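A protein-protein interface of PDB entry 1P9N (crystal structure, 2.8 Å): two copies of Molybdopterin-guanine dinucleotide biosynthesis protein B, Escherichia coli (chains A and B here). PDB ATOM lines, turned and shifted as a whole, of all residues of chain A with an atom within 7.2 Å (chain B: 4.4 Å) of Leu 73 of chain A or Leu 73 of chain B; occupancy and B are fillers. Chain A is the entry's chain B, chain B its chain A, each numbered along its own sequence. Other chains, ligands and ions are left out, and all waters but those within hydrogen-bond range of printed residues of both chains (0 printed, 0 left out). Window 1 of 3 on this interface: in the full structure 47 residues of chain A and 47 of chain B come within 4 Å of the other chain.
NE2 of Gln 62 of chain B lies within hydrogen-bond range of O of Asp 93 of chain A, at 2.8 Å.
The backbone carbonyl oxygen (O) of Trp 71 of chain B sits at hydrogen-bond distance from the backbone NH (N) of Thr 75 of chain A, 3.1 Å away.
N of Leu 73 of chain B lies within hydrogen-bond range of O of Leu 73 of chain A, 3.0 Å away.
The backbone NH (N) of Trp 71 of chain A lies within hydrogen-bond range of the backbone carbonyl oxygen (O) of Thr 75 of chain B, at 2.9 Å.
The backbone carbonyl oxygen (O) of Thr 63 of chain B is in hydrogen-bond range of the backbone NH (N) of Met 74 of chain B (2.8 Å).
O of Thr 63 of chain A is in hydrogen-bond range of N of Met 74 of chain A (2.8 Å).
O of Val 65 of chain A lies within hydrogen-bond range of N of Ala 72 of chain A, 2.8 Å away.
CB of Ala 72 of chain B touches CE of Met 43 of chain A, 3.5 Å away.
Trp 71 of chain A touches Leu 73 of chain B (O to O, 3.8 Å).
CA of Met 74 of chain B touches O of Trp 71 of chain A, at 3.9 Å.
Ala 72 of chain A touches Leu 73 of chain B.
Trp 71 of chain B touches Met 74 of chain A (O to CA, 3.7 Å).
Met 74 of chain A touches Ala 72 of chain B (SD to CB, 3.8 Å).
Leu 88 of chain A touches Ile 64 of chain B.
Met 92 of chain B touches Arg 91 of chain A.
OE1 of Gln 62 of chain B touches CB of Met 92 of chain A, at 3.5 Å.
Met 92 of chain A touches Ile 64 of chain B (SD to CG2, 3.4 Å).
Of the printed residues of chain B, Met 92 of chain A touches Gln 62, Ile 64 and Leu 73.
Printed residues of chain A within 4 Å of Gln 62 of chain B: Met 92 (3.5 Å) and Asp 93 (2.8 Å).
Of the printed residues of chain A, Leu 73 of chain B touches Trp 71, Ala 72, Leu 73, Arg 91 and Met 92.
Printed residues of chain A within 4 Å of Met 92 of chain B: Gln 62, Ile 64 and Arg 91.
The nearest residue of chain B that does not touch Leu 73 of chain A is Met 92 of chain B (4.1 Å).
The nearest residue of chain A that does not touch Leu 73 of chain B is Asp 93 of chain A (5.0 Å).
Of the 9 printed residues of chain B, 8 touch a printed residue of chain A.
Printed residues of chain B that touch a printed residue of chain A: Gln 62, Ile 64, Trp 71, Ala 72, Leu 73, Met 74, Thr 75 and Met 92.
Hydrophobic or aromatic side chains of chain B within 4 Å of the printed part of chain A: Ile 64, Trp 71, Ala 72, Leu 73 and Met 92.
Along chain B the printed residues that touch a printed residue of chain A span positions 62 to 92.
Of the 18 printed residues of chain A, 12 touch a printed residue of chain B.
Hydrophobic or aromatic side chains of chain A that line the printed part of chain B: Met 43, Ile 64, Trp 71, Leu 73, Met 74, Leu 88 and Met 92.
Trp 71 of chain A touches Leu 73 of chain B, and with the chains exchanged Leu 73 of chain A touches Trp 71 of chain B.
Trp 71 of chain A touches Met 74 of chain B, and with the chains exchanged Met 74 of chain A touches Trp 71 of chain B.
Leu 73 of chain B touches its own counterpart, Leu 73 of chain A.
Met 74 of chain A touches Ala 72 of chain B, but with the chains exchanged Ala 72 of chain A does not touch Met 74 of chain B (4.3 Å).
Positions printed for both chains: 62, 63, 64, 71, 72, 73, 74, 75 and 92.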
ATOM      1  N   MET A  43       7.204  -9.522  20.927  1.00  0.00           N
ATOM      2  CA  MET A  43       7.686 -10.681  21.684  1.00  0.00           C
ATOM      3  C   MET A  43       6.585 -11.389  22.467  1.00  0.00           C
ATOM      4  O   MET A  43       6.107 -12.447  22.066  1.00  0.00           O
ATOM      5  CB  MET A  43       8.791 -10.262  22.658  1.00  0.00           C
ATOM      6  CG  MET A  43       9.427  -8.897  22.380  1.00  0.00           C
ATOM      7  SD  MET A  43      10.433  -8.710  20.718  1.00  0.00           S
ATOM      8  CE  MET A  43      11.832 -10.028  21.081  1.00  0.00           C
ATOM      9  N   ASP A  51      11.138 -15.890  31.916  1.00  0.00           N
ATOM     10  CA  ASP A  51      12.447 -15.429  31.457  1.00  0.00           C
ATOM     11  C   ASP A  51      13.071 -14.547  32.547  1.00  0.00           C
ATOM     12  O   ASP A  51      14.113 -14.880  33.119  1.00  0.00           O
ATOM     13  CB  ASP A  51      12.297 -14.622  30.154  1.00  0.00           C
ATOM     14  CG  ASP A  51      13.517 -14.732  29.243  1.00  0.00           C
ATOM     15  OD1 ASP A  51      13.815 -15.856  28.777  1.00  0.00           O
ATOM     16  OD2 ASP A  51      14.172 -13.696  28.983  1.00  0.00           O
ATOM     17  N   ALA A  61      15.725  -1.385  32.119  1.00  0.00           N
ATOM     18  CA  ALA A  61      15.452  -1.216  30.698  1.00  0.00           C
ATOM     19  C   ALA A  61      16.126  -2.370  29.951  1.00  0.00           C
ATOM     20  O   ALA A  61      15.463  -3.195  29.321  1.00  0.00           O
ATOM     21  CB  ALA A  61      16.003   0.110  30.228  1.00  0.00           C
ATOM     22  N   GLN A  62      17.446  -2.435  30.059  1.00  0.00           N
ATOM     23  CA  GLN A  62      18.209  -3.489  29.420  1.00  0.00           C
ATOM     24  C   GLN A  62      18.446  -4.689  30.344  1.00  0.00           C
ATOM     25  O   GLN A  62      19.210  -4.605  31.295  1.00  0.00           O
ATOM     26  CB  GLN A  62      19.560  -2.941  28.936  1.00  0.00           C
ATOM     27  CG  GLN A  62      19.464  -1.781  27.951  1.00  0.00           C
ATOM     28  CD  GLN A  62      20.825  -1.241  27.519  1.00  0.00           C
ATOM     29  OE1 GLN A  62      21.593  -1.923  26.825  1.00  0.00           O
ATOM     30  NE2 GLN A  62      21.130  -0.011  27.931  1.00  0.00           N
ATOM     31  N   THR A  63      17.769  -5.800  30.068  1.00  0.00           N
ATOM     32  CA  THR A  63      17.967  -7.032  30.827  1.00  0.00           C
ATOM     33  C   THR A  63      18.731  -8.016  29.915  1.00  0.00           C
ATOM     34  O   THR A  63      18.751  -7.870  28.690  1.00  0.00           O
ATOM     35  CB  THR A  63      16.651  -7.682  31.224  1.00  0.00           C
ATOM     36  OG1 THR A  63      16.921  -8.741  32.148  1.00  0.00           O
ATOM     37  CG2 THR A  63      15.958  -8.278  30.003  1.00  0.00           C
ATOM     38  N   ILE A  64      19.338  -9.036  30.501  1.00  0.00           N
ATOM     39  CA  ILE A  64      20.112  -9.975  29.706  1.00  0.00           C
ATOM     40  C   ILE A  64      20.219 -11.320  30.398  1.00  0.00           C
ATOM     41  O   ILE A  64      20.881 -11.440  31.419  1.00  0.00           O
ATOM     42  CB  ILE A  64      21.502  -9.370  29.469  1.00  0.00           C
ATOM     43  CG1 ILE A  64      22.495 -10.405  28.967  1.00  0.00           C
ATOM     44  CG2 ILE A  64      21.972  -8.704  30.740  1.00  0.00           C
ATOM     45  CD1 ILE A  64      23.808  -9.763  28.569  1.00  0.00           C
ATOM     46  N   VAL A  65      19.559 -12.330  29.845  1.00  0.00           N
ATOM     47  CA  VAL A  65      19.581 -13.659  30.437  1.00  0.00           C
ATOM     48  C   VAL A  65      20.539 -14.568  29.702  1.00  0.00           C
ATOM     49  O   VAL A  65      20.436 -14.711  28.490  1.00  0.00           O
ATOM     50  CB  VAL A  65      18.209 -14.326  30.379  1.00  0.00           C
ATOM     51  CG1 VAL A  65      18.234 -15.616  31.163  1.00  0.00           C
ATOM     52  CG2 VAL A  65      17.154 -13.394  30.914  1.00  0.00           C
ATOM     53  N   TRP A  71      22.208 -16.968  25.006  1.00  0.00           N
ATOM     54  CA  TRP A  71      22.019 -15.782  25.832  1.00  0.00           C
ATOM     55  C   TRP A  71      21.251 -14.679  25.110  1.00  0.00           C
ATOM     56  O   TRP A  71      21.584 -14.298  23.990  1.00  0.00           O
ATOM     57  CB  TRP A  71      23.355 -15.230  26.364  1.00  0.00           C
ATOM     58  CG  TRP A  71      24.412 -14.733  25.367  1.00  0.00           C
ATOM     59  CD1 TRP A  71      25.569 -15.375  25.023  1.00  0.00           C
ATOM     60  CD2 TRP A  71      24.487 -13.437  24.752  1.00  0.00           C
ATOM     61  NE1 TRP A  71      26.363 -14.561  24.255  1.00  0.00           N
ATOM     62  CE2 TRP A  71      25.724 -13.369  24.069  1.00  0.00           C
ATOM     63  CE3 TRP A  71      23.635 -12.324  24.719  1.00  0.00           C
ATOM     64  CZ2 TRP A  71      26.129 -12.235  23.364  1.00  0.00           C
ATOM     65  CZ3 TRP A  71      24.041 -11.190  24.017  1.00  0.00           C
ATOM     66  CH2 TRP A  71      25.277 -11.156  23.350  1.00  0.00           C
ATOM     67  N   ALA A  72      20.213 -14.168  25.767  1.00  0.00           N
ATOM     68  CA  ALA A  72      19.387 -13.110  25.200  1.00  0.00           C
ATOM     69  C   ALA A  72      19.709 -11.754  25.795  1.00  0.00           C
ATOM     70  O   ALA A  72      20.250 -11.655  26.889  1.00  0.00           O
ATOM     71  CB  ALA A  72      17.932 -13.425  25.419  1.00  0.00           C
ATOM     72  N   LEU A  73      19.375 -10.709  25.053  1.00  0.00           N
ATOM     73  CA  LEU A  73      19.597  -9.343  25.482  1.00  0.00           C
ATOM     74  C   LEU A  73      18.373  -8.537  25.090  1.00  0.00           C
ATOM     75  O   LEU A  73      18.102  -8.340  23.915  1.00  0.00           O
ATOM     76  CB  LEU A  73      20.858  -8.765  24.823  1.00  0.00           C
ATOM     77  CG  LEU A  73      21.177  -7.257  24.900  1.00  0.00           C
ATOM     78  CD1 LEU A  73      20.409  -6.487  23.839  1.00  0.00           C
ATOM     79  CD2 LEU A  73      20.843  -6.727  26.278  1.00  0.00           C
ATOM     80  N   MET A  74      17.620  -8.092  26.088  1.00  0.00           N
ATOM     81  CA  MET A  74      16.426  -7.296  25.842  1.00  0.00           C
ATOM     82  C   MET A  74      16.734  -5.819  26.075  1.00  0.00           C
ATOM     83  O   MET A  74      17.523  -5.469  26.949  1.00  0.00           O
ATOM     84  CB  MET A  74      15.300  -7.739  26.768  1.00  0.00           C
ATOM     85  CG  MET A  74      13.971  -7.097  26.432  1.00  0.00           C
ATOM     86  SD  MET A  74      13.252  -7.613  24.679  1.00  0.00           S
ATOM     87  CE  MET A  74      12.001  -8.999  25.273  1.00  0.00           C
ATOM     88  N   THR A  75      16.118  -4.957  25.276  1.00  0.00           N
ATOM     89  CA  THR A  75      16.329  -3.520  25.390  1.00  0.00           C
ATOM     90  C   THR A  75      15.029  -2.781  25.123  1.00  0.00           C
ATOM     91  O   THR A  75      14.595  -2.676  23.980  1.00  0.00           O
ATOM     92  CB  THR A  75      17.399  -3.029  24.396  1.00  0.00           C
ATOM     93  OG1 THR A  75      18.693  -3.479  24.821  1.00  0.00           O
ATOM     94  CG2 THR A  75      17.386  -1.512  24.303  1.00  0.00           C
ATOM     95  N   LEU A  88      20.802  -1.585  14.866  1.00  0.00           N
ATOM     96  CA  LEU A  88      20.552  -2.946  15.320  1.00  0.00           C
ATOM     97  C   LEU A  88      21.694  -3.861  14.842  1.00  0.00           C
ATOM     98  O   LEU A  88      21.921  -4.940  15.389  1.00  0.00           O
ATOM     99  CB  LEU A  88      19.204  -3.437  14.791  1.00  0.00           C
ATOM    100  CG  LEU A  88      17.960  -2.705  15.313  1.00  0.00           C
ATOM    101  CD1 LEU A  88      16.705  -3.238  14.626  1.00  0.00           C
ATOM    102  CD2 LEU A  88      17.839  -2.896  16.807  1.00  0.00           C
ATOM    103  N   ALA A  89      22.421  -3.408  13.825  1.00  0.00           N
ATOM    104  CA  ALA A  89      23.554  -4.147  13.275  1.00  0.00           C
ATOM    105  C   ALA A  89      24.728  -4.073  14.243  1.00  0.00           C
ATOM    106  O   ALA A  89      25.172  -5.088  14.787  1.00  0.00           O
ATOM    107  CB  ALA A  89      23.966  -3.550  11.935  1.00  0.00           C
ATOM    108  N   SER A  90      25.229  -2.857  14.441  1.00  0.00           N
ATOM    109  CA  SER A  90      26.354  -2.589  15.335  1.00  0.00           C
ATOM    110  C   SER A  90      26.179  -3.281  16.684  1.00  0.00           C
ATOM    111  O   SER A  90      27.144  -3.492  17.430  1.00  0.00           O
ATOM    112  CB  SER A  90      26.486  -1.077  15.533  1.00  0.00           C
ATOM    113  OG  SER A  90      25.207  -0.486  15.682  1.00  0.00           O
ATOM    114  N   ARG A  91      24.938  -3.633  16.989  1.00  0.00           N
ATOM    115  CA  ARG A  91      24.630  -4.301  18.238  1.00  0.00           C
ATOM    116  C   ARG A  91      25.091  -5.758  18.234  1.00  0.00           C
ATOM    117  O   ARG A  91      25.462  -6.293  19.280  1.00  0.00           O
ATOM    118  CB  ARG A  91      23.119  -4.230  18.511  1.00  0.00           C
ATOM    119  CG  ARG A  91      22.599  -2.890  19.040  1.00  0.00           C
ATOM    120  CD  ARG A  91      23.107  -2.594  20.450  1.00  0.00           C
ATOM    121  NE  ARG A  91      24.430  -1.975  20.445  1.00  0.00           N
ATOM    122  CZ  ARG A  91      25.203  -1.860  21.521  1.00  0.00           C
ATOM    123  NH1 ARG A  91      24.778  -2.330  22.688  1.00  0.00           N
ATOM    124  NH2 ARG A  91      26.394  -1.276  21.429  1.00  0.00           N
ATOM    125  N   MET A  92      25.066  -6.391  17.062  1.00  0.00           N
ATOM    126  CA  MET A  92      25.463  -7.789  16.925  1.00  0.00           C
ATOM    127  C   MET A  92      26.959  -7.991  16.960  1.00  0.00           C
ATOM    128  O   MET A  92      27.730  -7.078  16.672  1.00  0.00           O
ATOM    129  CB  MET A  92      24.937  -8.375  15.618  1.00  0.00           C
ATOM    130  CG  MET A  92      23.445  -8.602  15.604  1.00  0.00           C
ATOM    131  SD  MET A  92      22.786  -9.121  13.838  1.00  0.00           S
ATOM    132  CE  MET A  92      24.058  -8.001  12.842  1.00  0.00           C
ATOM    133  N   ASP A  93      27.363  -9.199  17.329  1.00  0.00           N
ATOM    134  CA  ASP A  93      28.775  -9.542  17.352  1.00  0.00           C
ATOM    135  C   ASP A  93      29.085  -9.956  15.918  1.00  0.00           C
ATOM    136  O   ASP A  93      29.091 -11.143  15.583  1.00  0.00           O
ATOM    137  CB  ASP A  93      29.041 -10.709  18.296  1.00  0.00           C
ATOM    138  CG  ASP A  93      30.512 -11.018  18.414  1.00  0.00           C
ATOM    139  OD1 ASP A  93      30.889 -11.854  19.267  1.00  0.00           O
ATOM    140  OD2 ASP A  93      31.292 -10.418  17.646  1.00  0.00           O
ATOM    141  N   GLN B  62      22.922 -15.590  15.414  1.00  0.00           N
ATOM    142  CA  GLN B  62      22.452 -14.384  16.055  1.00  0.00           C
ATOM    143  C   GLN B  62      21.216 -13.844  15.364  1.00  0.00           C
ATOM    144  O   GLN B  62      21.280 -13.319  14.264  1.00  0.00           O
ATOM    145  CB  GLN B  62      23.553 -13.331  16.039  1.00  0.00           C
ATOM    146  CG  GLN B  62      24.806 -13.719  16.808  1.00  0.00           C
ATOM    147  CD  GLN B  62      25.850 -12.619  16.785  1.00  0.00           C
ATOM    148  OE1 GLN B  62      25.571 -11.480  17.137  1.00  0.00           O
ATOM    149  NE2 GLN B  62      27.056 -12.955  16.370  1.00  0.00           N
ATOM    150  N   THR B  63      20.084 -13.983  16.029  1.00  0.00           N
ATOM    151  CA  THR B  63      18.815 -13.493  15.522  1.00  0.00           C
ATOM    152  C   THR B  63      18.385 -12.310  16.411  1.00  0.00           C
ATOM    153  O   THR B  63      18.349 -12.431  17.631  1.00  0.00           O
ATOM    154  CB  THR B  63      17.757 -14.603  15.613  1.00  0.00           C
ATOM    155  OG1 THR B  63      18.291 -15.810  15.058  1.00  0.00           O
ATOM    156  CG2 THR B  63      16.503 -14.210  14.859  1.00  0.00           C
ATOM    157  N   ILE B  64      18.069 -11.168  15.814  1.00  0.00           N
ATOM    158  CA  ILE B  64      17.648 -10.012  16.603  1.00  0.00           C
ATOM    159  C   ILE B  64      16.275  -9.497  16.151  1.00  0.00           C
ATOM    160  O   ILE B  64      16.144  -8.829  15.130  1.00  0.00           O
ATOM    161  CB  ILE B  64      18.741  -8.894  16.562  1.00  0.00           C
ATOM    162  CG1 ILE B  64      18.168  -7.550  16.111  1.00  0.00           C
ATOM    163  CG2 ILE B  64      19.869  -9.328  15.648  1.00  0.00           C
ATOM    164  CD1 ILE B  64      19.195  -6.446  16.098  1.00  0.00           C
ATOM    165  N   TRP B  71      13.559  -4.448  21.556  1.00  0.00           N
ATOM    166  CA  TRP B  71      14.201  -5.446  20.698  1.00  0.00           C
ATOM    167  C   TRP B  71      15.158  -6.392  21.441  1.00  0.00           C
ATOM    168  O   TRP B  71      15.846  -5.997  22.391  1.00  0.00           O
ATOM    169  CB  TRP B  71      14.964  -4.753  19.589  1.00  0.00           C
ATOM    170  CG  TRP B  71      16.061  -3.898  20.090  1.00  0.00           C
ATOM    171  CD1 TRP B  71      15.986  -2.587  20.429  1.00  0.00           C
ATOM    172  CD2 TRP B  71      17.432  -4.265  20.207  1.00  0.00           C
ATOM    173  NE1 TRP B  71      17.233  -2.100  20.730  1.00  0.00           N
ATOM    174  CE2 TRP B  71      18.139  -3.112  20.600  1.00  0.00           C
ATOM    175  CE3 TRP B  71      18.132  -5.457  20.009  1.00  0.00           C
ATOM    176  CZ2 TRP B  71      19.513  -3.114  20.794  1.00  0.00           C
ATOM    177  CZ3 TRP B  71      19.494  -5.459  20.203  1.00  0.00           C
ATOM    178  CH2 TRP B  71      20.174  -4.290  20.591  1.00  0.00           C
ATOM    179  N   ALA B  72      15.221  -7.633  20.966  1.00  0.00           N
ATOM    180  CA  ALA B  72      16.055  -8.654  21.586  1.00  0.00           C
ATOM    181  C   ALA B  72      17.103  -9.267  20.668  1.00  0.00           C
ATOM    182  O   ALA B  72      16.784  -9.715  19.578  1.00  0.00           O
ATOM    183  CB  ALA B  72      15.164  -9.758  22.138  1.00  0.00           C
ATOM    184  N   LEU B  73      18.352  -9.295  21.113  1.00  0.00           N
ATOM    185  CA  LEU B  73      19.408  -9.909  20.331  1.00  0.00           C
ATOM    186  C   LEU B  73      19.638 -11.293  20.940  1.00  0.00           C
ATOM    187  O   LEU B  73      20.292 -11.411  21.965  1.00  0.00           O
ATOM    188  CB  LEU B  73      20.698  -9.095  20.422  1.00  0.00           C
ATOM    189  CG  LEU B  73      21.803  -9.456  19.407  1.00  0.00           C
ATOM    190  CD1 LEU B  73      23.050  -8.640  19.694  1.00  0.00           C
ATOM    191  CD2 LEU B  73      22.136 -10.928  19.462  1.00  0.00           C
ATOM    192  N   MET B  74      19.113 -12.341  20.315  1.00  0.00           N
ATOM    193  CA  MET B  74      19.287 -13.692  20.844  1.00  0.00           C
ATOM    194  C   MET B  74      20.461 -14.429  20.200  1.00  0.00           C
ATOM    195  O   MET B  74      20.463 -14.690  19.006  1.00  0.00           O
ATOM    196  CB  MET B  74      17.999 -14.470  20.648  1.00  0.00           C
ATOM    197  CG  MET B  74      16.819 -13.746  21.259  1.00  0.00           C
ATOM    198  SD  MET B  74      15.148 -13.918  20.273  1.00  0.00           S
ATOM    199  CE  MET B  74      14.363 -15.367  21.321  1.00  0.00           C
ATOM    200  N   THR B  75      21.458 -14.768  21.012  1.00  0.00           N
ATOM    201  CA  THR B  75      22.652 -15.455  20.540  1.00  0.00           C
ATOM    202  C   THR B  75      22.719 -16.924  20.967  1.00  0.00           C
ATOM    203  O   THR B  75      22.461 -17.246  22.125  1.00  0.00           O
ATOM    204  CB  THR B  75      23.920 -14.740  21.049  1.00  0.00           C
ATOM    205  OG1 THR B  75      23.909 -13.381  20.607  1.00  0.00           O
ATOM    206  CG2 THR B  75      25.164 -15.400  20.518  1.00  0.00           C
ATOM    207  N   MET B  92      25.855  -4.592  26.360  1.00  0.00           N
ATOM    208  CA  MET B  92      24.781  -3.653  26.682  1.00  0.00           C
ATOM    209  C   MET B  92      25.119  -2.258  26.237  1.00  0.00           C
ATOM    210  O   MET B  92      26.292  -1.904  26.054  1.00  0.00           O
ATOM    211  CB  MET B  92      24.487  -3.635  28.185  1.00  0.00           C
ATOM    212  CG  MET B  92      23.517  -4.708  28.607  1.00  0.00           C
ATOM    213  SD  MET B  92      23.552  -5.053  30.495  1.00  0.00           S
ATOM    214  CE  MET B  92      25.420  -4.583  30.757  1.00  0.00           C
